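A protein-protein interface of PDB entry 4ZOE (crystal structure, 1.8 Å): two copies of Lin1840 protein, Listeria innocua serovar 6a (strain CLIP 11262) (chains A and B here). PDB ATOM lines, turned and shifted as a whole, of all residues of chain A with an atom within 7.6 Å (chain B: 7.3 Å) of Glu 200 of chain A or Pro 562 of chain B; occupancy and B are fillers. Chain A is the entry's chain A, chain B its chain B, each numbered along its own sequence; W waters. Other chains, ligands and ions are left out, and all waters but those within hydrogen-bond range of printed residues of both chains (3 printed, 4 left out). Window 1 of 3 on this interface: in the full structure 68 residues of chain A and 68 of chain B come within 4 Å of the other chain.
Arg 146 of chain A touches Ile 561 of chain B, and with the chains exchanged Ile 561 of chain A touches Arg 146 of chain B. 3 positions are printed for both chains.
Of the 17 printed residues of chain B, 9 touch a printed residue of chain A. Printed residues of chain B that touch a printed residue of chain A: Arg 146, Glu 214, Gly 559, Gln 560, Ile 561, Pro 562, Tyr 564, Leu 568 and Tyr 587. Along chain B the printed residues that touch a printed residue of chain A span positions 146 to 587. Among the printed residues, 14 pairs touch across the chains.
The guanidinium group (NH2) of Arg 146 of chain A lies within salt-bridge range of the side-chain carboxylate (OD2) of Asp 144 of chain A. O of Glu 200 of chain A lies within hydrogen-bond range of ND2 of Asn 206 of chain A (2.9 Å). N of Glu 200 of chain A lies within hydrogen-bond range of O of Thr 207 of chain A. The side-chain hydroxyl of Ser 476 of chain A is in hydrogen-bond range of the backbone carbonyl oxygen of Gly 202 of chain A (2.7 Å). The backbone NH of Glu 204 of chain A lies within hydrogen-bond range of the side-chain hydroxyl of Ser 476 of chain A. OD2 of Asp 144 of chain B is in salt-bridge range of NH2 of Arg 146 of chain B, 2.8 Å away.
Of the printed residues of chain B, Ala 201 of chain A touches Gly 559 (3.9 Å), Gln 560 (3.7 Å), Ile 561 (3.6 Å), Pro 562 (3.9 Å) and Tyr 587 (2.7 Å). Of the printed residues of chain A, Ile 561 of chain B touches Arg 146 (3.1 Å) and Ala 201 (3.6 Å). Of chain A, only Glu 200 (3.3 Å) and Ala 201 (3.9 Å) come within 4 Å of Pro 562 of chain B. Of the printed residues of chain A, Tyr 587 of chain B touches Ala 201 (2.7 Å), Leu 203 (3.7 Å) and Ser 476 (3.6 Å). The nearest residue of chain A that does not touch Pro 562 of chain B is Arg 146 of chain A (5.3 Å). The nearest printed residue of chain A that does not touch Tyr 564 of chain B is Thr 207 of chain A (5.0 Å).
Among the printed residues, pairs that only touch across the chains: Glu 200 of chain A with Pro 562 of chain B (3.3 Å), Asn 209 of chain A with Glu 214 of chain B (3.3 Å), Thr 207 of chain A with Leu 568 of chain B (3.5 Å), Ala 201 of chain A with Ile 561 of chain B (3.6 Å), Ser 476 of chain A with Tyr 587 of chain B (3.6 Å), Leu 203 of chain A with Tyr 587 of chain B (3.7 Å), Ala 201 of chain A with Gln 560 of chain B (3.7 Å), Ala 201 of chain A with Gly 559 of chain B (3.9 Å) and Ala 201 of chain A with Pro 562 of chain B (3.9 Å).
Water W2 bridges OD1 of Asn 206 of chain A (2.6 Å) and O of Leu 568 of chain B (2.9 Å). Water W1 lies within hydrogen-bond range of OG1 of Thr 207 of chain A, N of Leu 568 of chain B and OH of Tyr 564 of chain B. Water W3 lies within hydrogen-bond range of OE2 of Glu 200 of chain A (2.8 Å) and NH1 of Arg 143 of chain B (3.0 Å).
NH1 of Arg 146 of chain A sits at hydrogen-bond distance from O of Gly 559 of chain B (2.8 Å). The backbone carbonyl oxygen (O) of Ile 561 of chain B lies within hydrogen-bond range of the guanidinium group (NH1) of Arg 146 of chain A (3.1 Å). The side-chain carboxylate of Glu 200 of chain A lies within hydrogen-bond range of the side-chain hydroxyl of Tyr 564 of chain B. O of Ala 201 of chain A lies within hydrogen-bond range of OH of Tyr 587 of chain B, at 2.7 Å. The backbone carbonyl oxygen of Ile 561 of chain A lies within hydrogen-bond range of the guanidinium group of Arg 146 of chain B.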
ATOM      1  N   ASP A 144      -4.144   0.989  25.810  1.00  0.00           N
ATOM      2  CA  ASP A 144      -4.875   0.679  24.544  1.00  0.00           C
ATOM      3  C   ASP A 144      -6.034   1.667  24.387  1.00  0.00           C
ATOM      4  O   ASP A 144      -7.144   1.485  24.874  1.00  0.00           O
ATOM      5  CB  ASP A 144      -5.299  -0.809  24.469  1.00  0.00           C
ATOM      6  CG  ASP A 144      -5.823  -1.187  23.089  1.00  0.00           C
ATOM      7  OD1 ASP A 144      -6.150  -0.264  22.281  1.00  0.00           O
ATOM      8  OD2 ASP A 144      -5.862  -2.403  22.850  1.00  0.00           O
ATOM      9  N   ARG A 146      -7.995   2.185  21.901  1.00  0.00           N
ATOM     10  CA  ARG A 146      -9.179   1.697  21.203  1.00  0.00           C
ATOM     11  C   ARG A 146     -10.296   1.573  22.249  1.00  0.00           C
ATOM     12  O   ARG A 146     -11.443   1.795  21.917  1.00  0.00           O
ATOM     13  CB  ARG A 146      -8.904   0.393  20.515  1.00  0.00           C
ATOM     14  CG  ARG A 146      -7.984   0.534  19.319  1.00  0.00           C
ATOM     15  CD  ARG A 146      -7.576  -0.853  18.785  1.00  0.00           C
ATOM     16  NE  ARG A 146      -6.652  -1.521  19.702  1.00  0.00           N
ATOM     17  CZ  ARG A 146      -5.939  -2.590  19.383  1.00  0.00           C
ATOM     18  NH1 ARG A 146      -6.093  -3.189  18.228  1.00  0.00           N
ATOM     19  NH2 ARG A 146      -5.112  -3.096  20.262  1.00  0.00           N
ATOM     20  N   TRP A 147      -9.957   1.182  23.479  1.00  0.00           N
ATOM     21  CA  TRP A 147     -10.932   0.906  24.515  1.00  0.00           C
ATOM     22  C   TRP A 147     -11.541   2.240  24.928  1.00  0.00           C
ATOM     23  O   TRP A 147     -10.844   3.201  25.343  1.00  0.00           O
ATOM     24  CB  TRP A 147     -10.239   0.260  25.721  1.00  0.00           C
ATOM     25  CG  TRP A 147     -11.166  -0.388  26.748  1.00  0.00           C
ATOM     26  CD1 TRP A 147     -12.097  -1.297  26.548  1.00  0.00           C
ATOM     27  CD2 TRP A 147     -11.007  -0.261  28.140  1.00  0.00           C
ATOM     28  NE1 TRP A 147     -12.502  -1.824  27.705  1.00  0.00           N
ATOM     29  CE2 TRP A 147     -11.884  -1.193  28.723  1.00  0.00           C
ATOM     30  CE3 TRP A 147     -10.163   0.503  28.941  1.00  0.00           C
ATOM     31  CZ2 TRP A 147     -12.118  -1.271  30.105  1.00  0.00           C
ATOM     32  CZ3 TRP A 147     -10.327   0.388  30.393  1.00  0.00           C
ATOM     33  CH2 TRP A 147     -11.304  -0.539  30.929  1.00  0.00           C
ATOM     34  N   TYR A 196      -9.110  -4.933  33.955  1.00  0.00           N
ATOM     35  CA  TYR A 196     -10.098  -4.770  32.908  1.00  0.00           C
ATOM     36  C   TYR A 196      -9.589  -3.978  31.689  1.00  0.00           C
ATOM     37  O   TYR A 196     -10.073  -4.239  30.564  1.00  0.00           O
ATOM     38  CB  TYR A 196     -11.399  -4.135  33.592  1.00  0.00           C
ATOM     39  CG  TYR A 196     -12.596  -3.835  32.826  1.00  0.00           C
ATOM     40  CD1 TYR A 196     -13.039  -4.613  31.773  1.00  0.00           C
ATOM     41  CD2 TYR A 196     -13.377  -2.716  33.118  1.00  0.00           C
ATOM     42  CE1 TYR A 196     -14.199  -4.297  31.062  1.00  0.00           C
ATOM     43  CE2 TYR A 196     -14.531  -2.478  32.430  1.00  0.00           C
ATOM     44  CZ  TYR A 196     -14.937  -3.240  31.405  1.00  0.00           C
ATOM     45  OH  TYR A 196     -16.081  -2.933  30.667  1.00  0.00           O
ATOM     46  N   GLY A 197      -8.705  -2.999  31.901  1.00  0.00           N
ATOM     47  CA  GLY A 197      -8.209  -2.169  30.798  1.00  0.00           C
ATOM     48  C   GLY A 197      -7.283  -2.885  29.840  1.00  0.00           C
ATOM     49  O   GLY A 197      -6.914  -2.224  28.791  1.00  0.00           O
ATOM     50  N   ALA A 198      -6.952  -4.144  30.119  1.00  0.00           N
ATOM     51  CA  ALA A 198      -6.038  -4.889  29.205  1.00  0.00           C
ATOM     52  C   ALA A 198      -6.858  -5.671  28.134  1.00  0.00           C
ATOM     53  O   ALA A 198      -6.351  -6.570  27.415  1.00  0.00           O
ATOM     54  CB  ALA A 198      -5.137  -5.737  29.995  1.00  0.00           C
ATOM     55  N   ALA A 199      -8.139  -5.359  28.032  1.00  0.00           N
ATOM     56  CA  ALA A 199      -9.018  -5.988  27.052  1.00  0.00           C
ATOM     57  C   ALA A 199      -8.304  -6.124  25.698  1.00  0.00           C
ATOM     58  O   ALA A 199      -7.818  -5.130  25.080  1.00  0.00           O
ATOM     59  CB  ALA A 199     -10.367  -5.235  26.914  1.00  0.00           C
ATOM     60  N   GLU A 200      -8.284  -7.366  25.212  1.00  0.00           N
ATOM     61  CA  GLU A 200      -7.619  -7.657  23.968  1.00  0.00           C
ATOM     62  C   GLU A 200      -8.262  -6.871  22.791  1.00  0.00           C
ATOM     63  O   GLU A 200      -9.488  -6.795  22.690  1.00  0.00           O
ATOM     64  CB  GLU A 200      -7.697  -9.140  23.600  1.00  0.00           C
ATOM     65  CG  GLU A 200      -6.661  -9.651  22.588  1.00  0.00           C
ATOM     66  CD  GLU A 200      -6.415 -11.163  22.835  1.00  0.00           C
ATOM     67  OE1 GLU A 200      -7.214 -11.792  22.194  1.00  0.00           O
ATOM     68  OE2 GLU A 200      -5.498 -11.679  23.664  1.00  0.00           O
ATOM     69  N   ALA A 201      -7.367  -6.308  21.976  1.00  0.00           N
ATOM     70  CA  ALA A 201      -7.668  -5.507  20.748  1.00  0.00           C
ATOM     71  C   ALA A 201      -8.575  -4.292  21.049  1.00  0.00           C
ATOM     72  O   ALA A 201      -9.301  -3.811  20.186  1.00  0.00           O
ATOM     73  CB  ALA A 201      -8.346  -6.440  19.755  1.00  0.00           C
ATOM     74  N   GLY A 202      -8.506  -3.806  22.303  1.00  0.00           N
ATOM     75  CA  GLY A 202      -9.365  -2.768  22.857  1.00  0.00           C
ATOM     76  C   GLY A 202     -10.856  -2.984  22.737  1.00  0.00           C
ATOM     77  O   GLY A 202     -11.619  -2.053  22.827  1.00  0.00           O
ATOM     78  N   LEU A 203     -11.260  -4.243  22.600  1.00  0.00           N
ATOM     79  CA  LEU A 203     -12.682  -4.587  22.392  1.00  0.00           C
ATOM     80  C   LEU A 203     -13.399  -4.733  23.714  1.00  0.00           C
ATOM     81  O   LEU A 203     -13.000  -5.453  24.603  1.00  0.00           O
ATOM     82  CB  LEU A 203     -12.846  -5.904  21.605  1.00  0.00           C
ATOM     83  CG  LEU A 203     -14.200  -6.561  21.328  1.00  0.00           C
ATOM     84  CD1 LEU A 203     -15.185  -5.654  20.598  1.00  0.00           C
ATOM     85  CD2 LEU A 203     -13.967  -7.864  20.561  1.00  0.00           C
ATOM     86  N   GLU A 204     -14.511  -4.026  23.819  1.00  0.00           N
ATOM     87  CA  GLU A 204     -15.225  -4.062  25.154  1.00  0.00           C
ATOM     88  C   GLU A 204     -15.472  -5.444  25.675  1.00  0.00           C
ATOM     89  O   GLU A 204     -15.991  -6.302  24.966  1.00  0.00           O
ATOM     90  CB  GLU A 204     -16.540  -3.301  25.074  1.00  0.00           C
ATOM     91  CG  GLU A 204     -17.039  -2.982  26.418  1.00  0.00           C
ATOM     92  CD  GLU A 204     -16.091  -2.189  27.256  1.00  0.00           C
ATOM     93  OE1 GLU A 204     -16.020  -0.911  27.169  1.00  0.00           O
ATOM     94  OE2 GLU A 204     -15.399  -2.814  28.103  1.00  0.00           O
ATOM     95  N   TYR A 205     -15.175  -5.651  26.971  1.00  0.00           N
ATOM     96  CA  TYR A 205     -15.428  -6.901  27.720  1.00  0.00           C
ATOM     97  C   TYR A 205     -14.559  -8.049  27.296  1.00  0.00           C
ATOM     98  O   TYR A 205     -14.794  -9.188  27.749  1.00  0.00           O
ATOM     99  CB  TYR A 205     -16.884  -7.382  27.716  1.00  0.00           C
ATOM    100  CG  TYR A 205     -17.972  -6.278  27.851  1.00  0.00           C
ATOM    101  CD1 TYR A 205     -18.015  -5.478  28.976  1.00  0.00           C
ATOM    102  CD2 TYR A 205     -18.837  -5.967  26.769  1.00  0.00           C
ATOM    103  CE1 TYR A 205     -18.967  -4.499  29.114  1.00  0.00           C
ATOM    104  CE2 TYR A 205     -19.838  -5.025  26.919  1.00  0.00           C
ATOM    105  CZ  TYR A 205     -19.868  -4.257  28.066  1.00  0.00           C
ATOM    106  OH  TYR A 205     -20.796  -3.246  28.326  1.00  0.00           O
ATOM    107  N   ASN A 206     -13.622  -7.814  26.393  1.00  0.00           N
ATOM    108  CA  ASN A 206     -12.921  -8.903  25.753  1.00  0.00           C
ATOM    109  C   ASN A 206     -11.841  -9.506  26.673  1.00  0.00           C
ATOM    110  O   ASN A 206     -11.434  -8.908  27.699  1.00  0.00           O
ATOM    111  CB  ASN A 206     -12.245  -8.440  24.452  1.00  0.00           C
ATOM    112  CG  ASN A 206     -11.922  -9.567  23.518  1.00  0.00           C
ATOM    113  OD1 ASN A 206     -12.429 -10.692  23.639  1.00  0.00           O
ATOM    114  ND2 ASN A 206     -11.008  -9.276  22.571  1.00  0.00           N
ATOM    115  N   THR A 207     -11.381 -10.687  26.288  1.00  0.00           N
ATOM    116  CA  THR A 207     -10.273 -11.399  27.012  1.00  0.00           C
ATOM    117  C   THR A 207      -9.137 -10.504  27.501  1.00  0.00           C
ATOM    118  O   THR A 207      -8.662  -9.631  26.815  1.00  0.00           O
ATOM    119  CB  THR A 207      -9.781 -12.466  26.092  1.00  0.00           C
ATOM    120  OG1 THR A 207     -10.916 -13.265  25.683  1.00  0.00           O
ATOM    121  CG2 THR A 207      -8.599 -13.314  26.711  1.00  0.00           C
ATOM    122  N   VAL A 208      -8.712 -10.741  28.740  1.00  0.00           N
ATOM    123  CA  VAL A 208      -7.529 -10.168  29.380  1.00  0.00           C
ATOM    124  C   VAL A 208      -6.619 -11.346  29.735  1.00  0.00           C
ATOM    125  O   VAL A 208      -7.106 -12.350  30.309  1.00  0.00           O
ATOM    126  CB  VAL A 208      -7.918  -9.380  30.655  1.00  0.00           C
ATOM    127  CG1 VAL A 208      -6.704  -9.058  31.543  1.00  0.00           C
ATOM    128  CG2 VAL A 208      -8.619  -8.098  30.208  1.00  0.00           C
ATOM    129  N   ASN A 209      -5.364 -11.248  29.349  1.00  0.00           N
ATOM    130  CA  ASN A 209      -4.374 -12.267  29.796  1.00  0.00           C
ATOM    131  C   ASN A 209      -3.009 -11.657  29.953  1.00  0.00           C
ATOM    132  O   ASN A 209      -2.571 -10.966  29.044  1.00  0.00           O
ATOM    133  CB  ASN A 209      -4.254 -13.436  28.818  1.00  0.00           C
ATOM    134  CG  ASN A 209      -3.344 -14.546  29.325  1.00  0.00           C
ATOM    135  OD1 ASN A 209      -2.135 -14.670  28.915  1.00  0.00           O
ATOM    136  ND2 ASN A 209      -3.908 -15.409  30.144  1.00  0.00           N
ATOM    137  N   SER A 476     -15.831   1.063  21.876  1.00  0.00           N
ATOM    138  CA  SER A 476     -14.511   0.644  21.312  1.00  0.00           C
ATOM    139  C   SER A 476     -14.408   1.114  19.873  1.00  0.00           C
ATOM    140  O   SER A 476     -15.310   0.816  19.043  1.00  0.00           O
ATOM    141  CB  SER A 476     -14.402  -0.901  21.382  1.00  0.00           C
ATOM    142  OG  SER A 476     -14.243  -1.435  22.735  1.00  0.00           O
ATOM    143  N   ILE A 561      -0.220   0.403  18.614  1.00  0.00           N
ATOM    144  CA  ILE A 561      -0.796   0.044  19.949  1.00  0.00           C
ATOM    145  C   ILE A 561      -0.482  -1.430  20.318  1.00  0.00           C
ATOM    146  O   ILE A 561      -0.666  -2.349  19.457  1.00  0.00           O
ATOM    147  CB  ILE A 561      -2.297   0.234  19.924  1.00  0.00           C
ATOM    148  CG1 ILE A 561      -2.585   1.708  19.750  1.00  0.00           C
ATOM    149  CG2 ILE A 561      -2.990  -0.344  21.191  1.00  0.00           C
ATOM    150  CD1 ILE A 561      -4.075   1.943  19.482  1.00  0.00           C
ATOM    151  N   ARG B 143      -0.822 -14.670  16.054  1.00  0.00           N
ATOM    152  CA  ARG B 143      -2.106 -13.995  16.002  1.00  0.00           C
ATOM    153  C   ARG B 143      -2.043 -12.540  15.544  1.00  0.00           C
ATOM    154  O   ARG B 143      -3.099 -11.816  15.668  1.00  0.00           O
ATOM    155  CB  ARG B 143      -2.744 -14.009  17.363  1.00  0.00           C
ATOM    156  CG  ARG B 143      -2.973 -15.393  17.948  1.00  0.00           C
ATOM    157  CD  ARG B 143      -3.568 -15.280  19.320  1.00  0.00           C
ATOM    158  NE  ARG B 143      -4.125 -16.571  19.755  1.00  0.00           N
ATOM    159  CZ  ARG B 143      -4.513 -16.839  20.994  1.00  0.00           C
ATOM    160  NH1 ARG B 143      -4.375 -15.944  21.975  1.00  0.00           N
ATOM    161  NH2 ARG B 143      -4.999 -18.039  21.269  1.00  0.00           N
ATOM    162  N   ASP B 144      -0.874 -12.116  15.054  1.00  0.00           N
ATOM    163  CA  ASP B 144      -0.588 -10.667  14.812  1.00  0.00           C
ATOM    164  C   ASP B 144       0.151 -10.539  13.499  1.00  0.00           C
ATOM    165  O   ASP B 144       1.340 -10.651  13.436  1.00  0.00           O
ATOM    166  CB  ASP B 144       0.158 -10.044  15.999  1.00  0.00           C
ATOM    167  CG  ASP B 144       0.247  -8.552  15.902  1.00  0.00           C
ATOM    168  OD1 ASP B 144       0.041  -7.989  14.809  1.00  0.00           O
ATOM    169  OD2 ASP B 144       0.524  -7.922  16.909  1.00  0.00           O
ATOM    170  N   PRO B 145      -0.612 -10.315  12.425  1.00  0.00           N
ATOM    171  CA  PRO B 145      -0.042 -10.106  11.139  1.00  0.00           C
ATOM    172  C   PRO B 145       0.843  -8.834  10.875  1.00  0.00           C
ATOM    173  O   PRO B 145       1.526  -8.757   9.839  1.00  0.00           O
ATOM    174  CB  PRO B 145      -1.269 -10.204  10.190  1.00  0.00           C
ATOM    175  CG  PRO B 145      -2.379  -9.810  10.973  1.00  0.00           C
ATOM    176  CD  PRO B 145      -2.060 -10.094  12.448  1.00  0.00           C
ATOM    177  N   ARG B 146       0.980  -7.925  11.835  1.00  0.00           N
ATOM    178  CA  ARG B 146       1.970  -6.875  11.755  1.00  0.00           C
ATOM    179  C   ARG B 146       3.364  -7.496  11.759  1.00  0.00           C
ATOM    180  O   ARG B 146       4.257  -6.958  11.094  1.00  0.00           O
ATOM    181  CB  ARG B 146       1.859  -5.902  12.917  1.00  0.00           C
ATOM    182  CG  ARG B 146       0.585  -5.128  12.844  1.00  0.00           C
ATOM    183  CD  ARG B 146       0.309  -4.351  14.104  1.00  0.00           C
ATOM    184  NE  ARG B 146      -0.028  -5.135  15.227  1.00  0.00           N
ATOM    185  CZ  ARG B 146      -0.553  -4.670  16.362  1.00  0.00           C
ATOM    186  NH1 ARG B 146      -0.674  -3.377  16.654  1.00  0.00           N
ATOM    187  NH2 ARG B 146      -0.808  -5.525  17.308  1.00  0.00           N
ATOM    188  N   GLU B 214      -1.591 -20.042  29.674  1.00  0.00           N
ATOM    189  CA  GLU B 214      -1.891 -19.752  28.291  1.00  0.00           C
ATOM    190  C   GLU B 214      -0.665 -20.255  27.478  1.00  0.00           C
ATOM    191  O   GLU B 214      -0.778 -20.759  26.366  1.00  0.00           O
ATOM    192  CB  GLU B 214      -2.000 -18.282  28.047  1.00  0.00           C
ATOM    193  CG  GLU B 214      -3.430 -17.828  27.908  1.00  0.00           C
ATOM    194  CD  GLU B 214      -4.225 -18.634  26.851  1.00  0.00           C
ATOM    195  OE1 GLU B 214      -5.218 -19.372  27.266  1.00  0.00           O
ATOM    196  OE2 GLU B 214      -3.875 -18.464  25.651  1.00  0.00           O
ATOM    197  N   TYR B 219       0.777 -21.980  23.286  1.00  0.00           N
ATOM    198  CA  TYR B 219       2.034 -21.545  22.684  1.00  0.00           C
ATOM    199  C   TYR B 219       3.060 -22.650  22.692  1.00  0.00           C
ATOM    200  O   TYR B 219       3.943 -22.635  21.850  1.00  0.00           O
ATOM    201  CB  TYR B 219       2.592 -20.314  23.393  1.00  0.00           C
ATOM    202  CG  TYR B 219       1.809 -19.094  22.946  1.00  0.00           C
ATOM    203  CD1 TYR B 219       0.585 -18.765  23.528  1.00  0.00           C
ATOM    204  CD2 TYR B 219       2.244 -18.307  21.918  1.00  0.00           C
ATOM    205  CE1 TYR B 219      -0.141 -17.673  23.041  1.00  0.00           C
ATOM    206  CE2 TYR B 219       1.494 -17.241  21.439  1.00  0.00           C
ATOM    207  CZ  TYR B 219       0.318 -16.924  22.047  1.00  0.00           C
ATOM    208  OH  TYR B 219      -0.442 -15.856  21.531  1.00  0.00           O
ATOM    209  N   PRO B 555      -7.925  -9.761   9.065  1.00  0.00           N
ATOM    210  CA  PRO B 555      -8.711  -8.761   9.789  1.00  0.00           C
ATOM    211  C   PRO B 555      -9.462  -7.759   8.881  1.00  0.00           C
ATOM    212  O   PRO B 555      -9.128  -7.497   7.757  1.00  0.00           O
ATOM    213  CB  PRO B 555      -7.662  -8.007  10.670  1.00  0.00           C
ATOM    214  CG  PRO B 555      -6.396  -8.884  10.618  1.00  0.00           C
ATOM    215  CD  PRO B 555      -6.471  -9.645   9.342  1.00  0.00           C
ATOM    216  N   THR B 558      -6.463  -3.082  10.626  1.00  0.00           N
ATOM    217  CA  THR B 558      -5.288  -3.250  11.460  1.00  0.00           C
ATOM    218  C   THR B 558      -5.682  -3.251  12.961  1.00  0.00           C
ATOM    219  O   THR B 558      -5.297  -4.139  13.726  1.00  0.00           O
ATOM    220  CB  THR B 558      -4.273  -2.138  11.161  1.00  0.00           C
ATOM    221  OG1 THR B 558      -3.666  -2.323   9.848  1.00  0.00           O
ATOM    222  CG2 THR B 558      -3.088  -2.212  12.152  1.00  0.00           C
ATOM    223  N   GLY B 559      -6.542  -2.311  13.338  1.00  0.00           N
ATOM    224  CA  GLY B 559      -6.968  -2.172  14.724  1.00  0.00           C
ATOM    225  C   GLY B 559      -7.884  -3.297  15.278  1.00  0.00           C
ATOM    226  O   GLY B 559      -8.276  -3.243  16.455  1.00  0.00           O
ATOM    227  N   GLN B 560      -8.301  -4.256  14.439  1.00  0.00           N
ATOM    228  CA  GLN B 560      -8.972  -5.474  14.984  1.00  0.00           C
ATOM    229  C   GLN B 560      -7.993  -6.486  15.574  1.00  0.00           C
ATOM    230  O   GLN B 560      -8.361  -7.489  16.160  1.00  0.00           O
ATOM    231  CB  GLN B 560      -9.778  -6.170  13.882  1.00  0.00           C
ATOM    232  CG  GLN B 560     -10.862  -7.117  14.338  1.00  0.00           C
ATOM    233  CD  GLN B 560     -11.638  -7.711  13.121  1.00  0.00           C
ATOM    234  OE1 GLN B 560     -11.020  -8.079  12.098  1.00  0.00           O
ATOM    235  NE2 GLN B 560     -12.936  -7.751  13.227  1.00  0.00           N
ATOM    236  N   ILE B 561      -6.727  -6.255  15.308  1.00  0.00           N
ATOM    237  CA  ILE B 561      -5.712  -7.232  15.723  1.00  0.00           C
ATOM    238  C   ILE B 561      -5.462  -7.227  17.240  1.00  0.00           C
ATOM    239  O   ILE B 561      -5.351  -6.124  17.843  1.00  0.00           O
ATOM    240  CB  ILE B 561      -4.402  -6.889  15.041  1.00  0.00           C
ATOM    241  CG1 ILE B 561      -4.483  -7.167  13.539  1.00  0.00           C
ATOM    242  CG2 ILE B 561      -3.296  -7.633  15.685  1.00  0.00           C
ATOM    243  CD1 ILE B 561      -3.290  -6.641  12.832  1.00  0.00           C
ATOM    244  N   PRO B 562      -5.408  -8.406  17.885  1.00  0.00           N
ATOM    245  CA  PRO B 562      -5.570  -9.746  17.382  1.00  0.00           C
ATOM    246  C   PRO B 562      -6.983 -10.260  17.265  1.00  0.00           C
ATOM    247  O   PRO B 562      -7.815 -10.138  18.177  1.00  0.00           O
ATOM    248  CB  PRO B 562      -4.792 -10.589  18.388  1.00  0.00           C
ATOM    249  CG  PRO B 562      -5.190  -9.969  19.700  1.00  0.00           C
ATOM    250  CD  PRO B 562      -5.027  -8.472  19.330  1.00  0.00           C
ATOM    251  N   VAL B 563      -7.239 -10.868  16.125  1.00  0.00           N
ATOM    252  CA  VAL B 563      -8.483 -11.507  15.811  1.00  0.00           C
ATOM    253  C   VAL B 563      -8.218 -12.934  15.321  1.00  0.00           C
ATOM    254  O   VAL B 563      -7.268 -13.170  14.523  1.00  0.00           O
ATOM    255  CB  VAL B 563      -9.276 -10.676  14.778  1.00  0.00           C
ATOM    256  CG1 VAL B 563      -8.537 -10.569  13.459  1.00  0.00           C
ATOM    257  CG2 VAL B 563     -10.665 -11.270  14.606  1.00  0.00           C
ATOM    258  N   TYR B 564      -8.966 -13.896  15.869  1.00  0.00           N
ATOM    259  CA  TYR B 564      -8.598 -15.304  15.678  1.00  0.00           C
ATOM    260  C   TYR B 564      -9.788 -16.156  16.024  1.00  0.00           C
ATOM    261  O   TYR B 564     -10.692 -15.751  16.820  1.00  0.00           O
ATOM    262  CB  TYR B 564      -7.291 -15.756  16.434  1.00  0.00           C
ATOM    263  CG  TYR B 564      -7.283 -15.385  17.897  1.00  0.00           C
ATOM    264  CD1 TYR B 564      -6.792 -14.130  18.349  1.00  0.00           C
ATOM    265  CD2 TYR B 564      -7.918 -16.192  18.852  1.00  0.00           C
ATOM    266  CE1 TYR B 564      -6.818 -13.815  19.709  1.00  0.00           C
ATOM    267  CE2 TYR B 564      -7.915 -15.888  20.191  1.00  0.00           C
ATOM    268  CZ  TYR B 564      -7.395 -14.699  20.631  1.00  0.00           C
ATOM    269  OH  TYR B 564      -7.540 -14.385  21.993  1.00  0.00           O
ATOM    270  N   HIS B 567     -11.454 -18.052  20.024  1.00  0.00           N
ATOM    271  CA  HIS B 567     -11.463 -16.999  20.981  1.00  0.00           C
ATOM    272  C   HIS B 567     -12.461 -17.311  22.087  1.00  0.00           C
ATOM    273  O   HIS B 567     -13.314 -18.170  21.895  1.00  0.00           O
ATOM    274  CB  HIS B 567     -11.831 -15.683  20.243  1.00  0.00           C
ATOM    275  CG  HIS B 567     -13.188 -15.740  19.618  1.00  0.00           C
ATOM    276  ND1 HIS B 567     -14.323 -15.511  20.356  1.00  0.00           N
ATOM    277  CD2 HIS B 567     -13.622 -15.998  18.359  1.00  0.00           C
ATOM    278  CE1 HIS B 567     -15.390 -15.660  19.600  1.00  0.00           C
ATOM    279  NE2 HIS B 567     -15.010 -15.946  18.394  1.00  0.00           N
ATOM    280  N   LEU B 568     -12.309 -16.629  23.219  1.00  0.00           N
ATOM    281  CA  LEU B 568     -13.231 -16.752  24.340  1.00  0.00           C
ATOM    282  C   LEU B 568     -14.550 -16.012  24.052  1.00  0.00           C
ATOM    283  O   LEU B 568     -14.639 -15.095  23.168  1.00  0.00           O
ATOM    284  CB  LEU B 568     -12.564 -16.314  25.627  1.00  0.00           C
ATOM    285  CG  LEU B 568     -11.148 -16.965  25.928  1.00  0.00           C
ATOM    286  CD1 LEU B 568     -10.800 -16.505  27.347  1.00  0.00           C
ATOM    287  CD2 LEU B 568     -11.070 -18.506  25.847  1.00  0.00           C
ATOM    288  N   TYR B 587     -17.312  -3.533  18.381  1.00  0.00           N
ATOM    289  CA  TYR B 587     -16.755  -2.275  17.995  1.00  0.00           C
ATOM    290  C   TYR B 587     -17.831  -1.331  17.372  1.00  0.00           C
ATOM    291  O   TYR B 587     -18.734  -1.782  16.641  1.00  0.00           O
ATOM    292  CB  TYR B 587     -15.694  -2.436  16.931  1.00  0.00           C
ATOM    293  CG  TYR B 587     -14.408  -3.120  17.350  1.00  0.00           C
ATOM    294  CD1 TYR B 587     -13.451  -2.461  18.105  1.00  0.00           C
ATOM    295  CD2 TYR B 587     -14.227  -4.459  17.084  1.00  0.00           C
ATOM    296  CE1 TYR B 587     -12.203  -3.096  18.417  1.00  0.00           C
ATOM    297  CE2 TYR B 587     -13.050  -5.103  17.399  1.00  0.00           C
ATOM    298  CZ  TYR B 587     -12.048  -4.418  18.117  1.00  0.00           C
ATOM    299  OH  TYR B 587     -10.880  -5.115  18.413  1.00  0.00           O
HETATM  300  O   HOH W   1     -10.199 -14.476  23.434  1.00  0.00           O
HETATM  301  O   HOH W   2     -12.872 -12.931  22.399  1.00  0.00           O
HETATM  302  O   HOH W   3      -3.728 -12.996  22.022  1.00  0.00           O
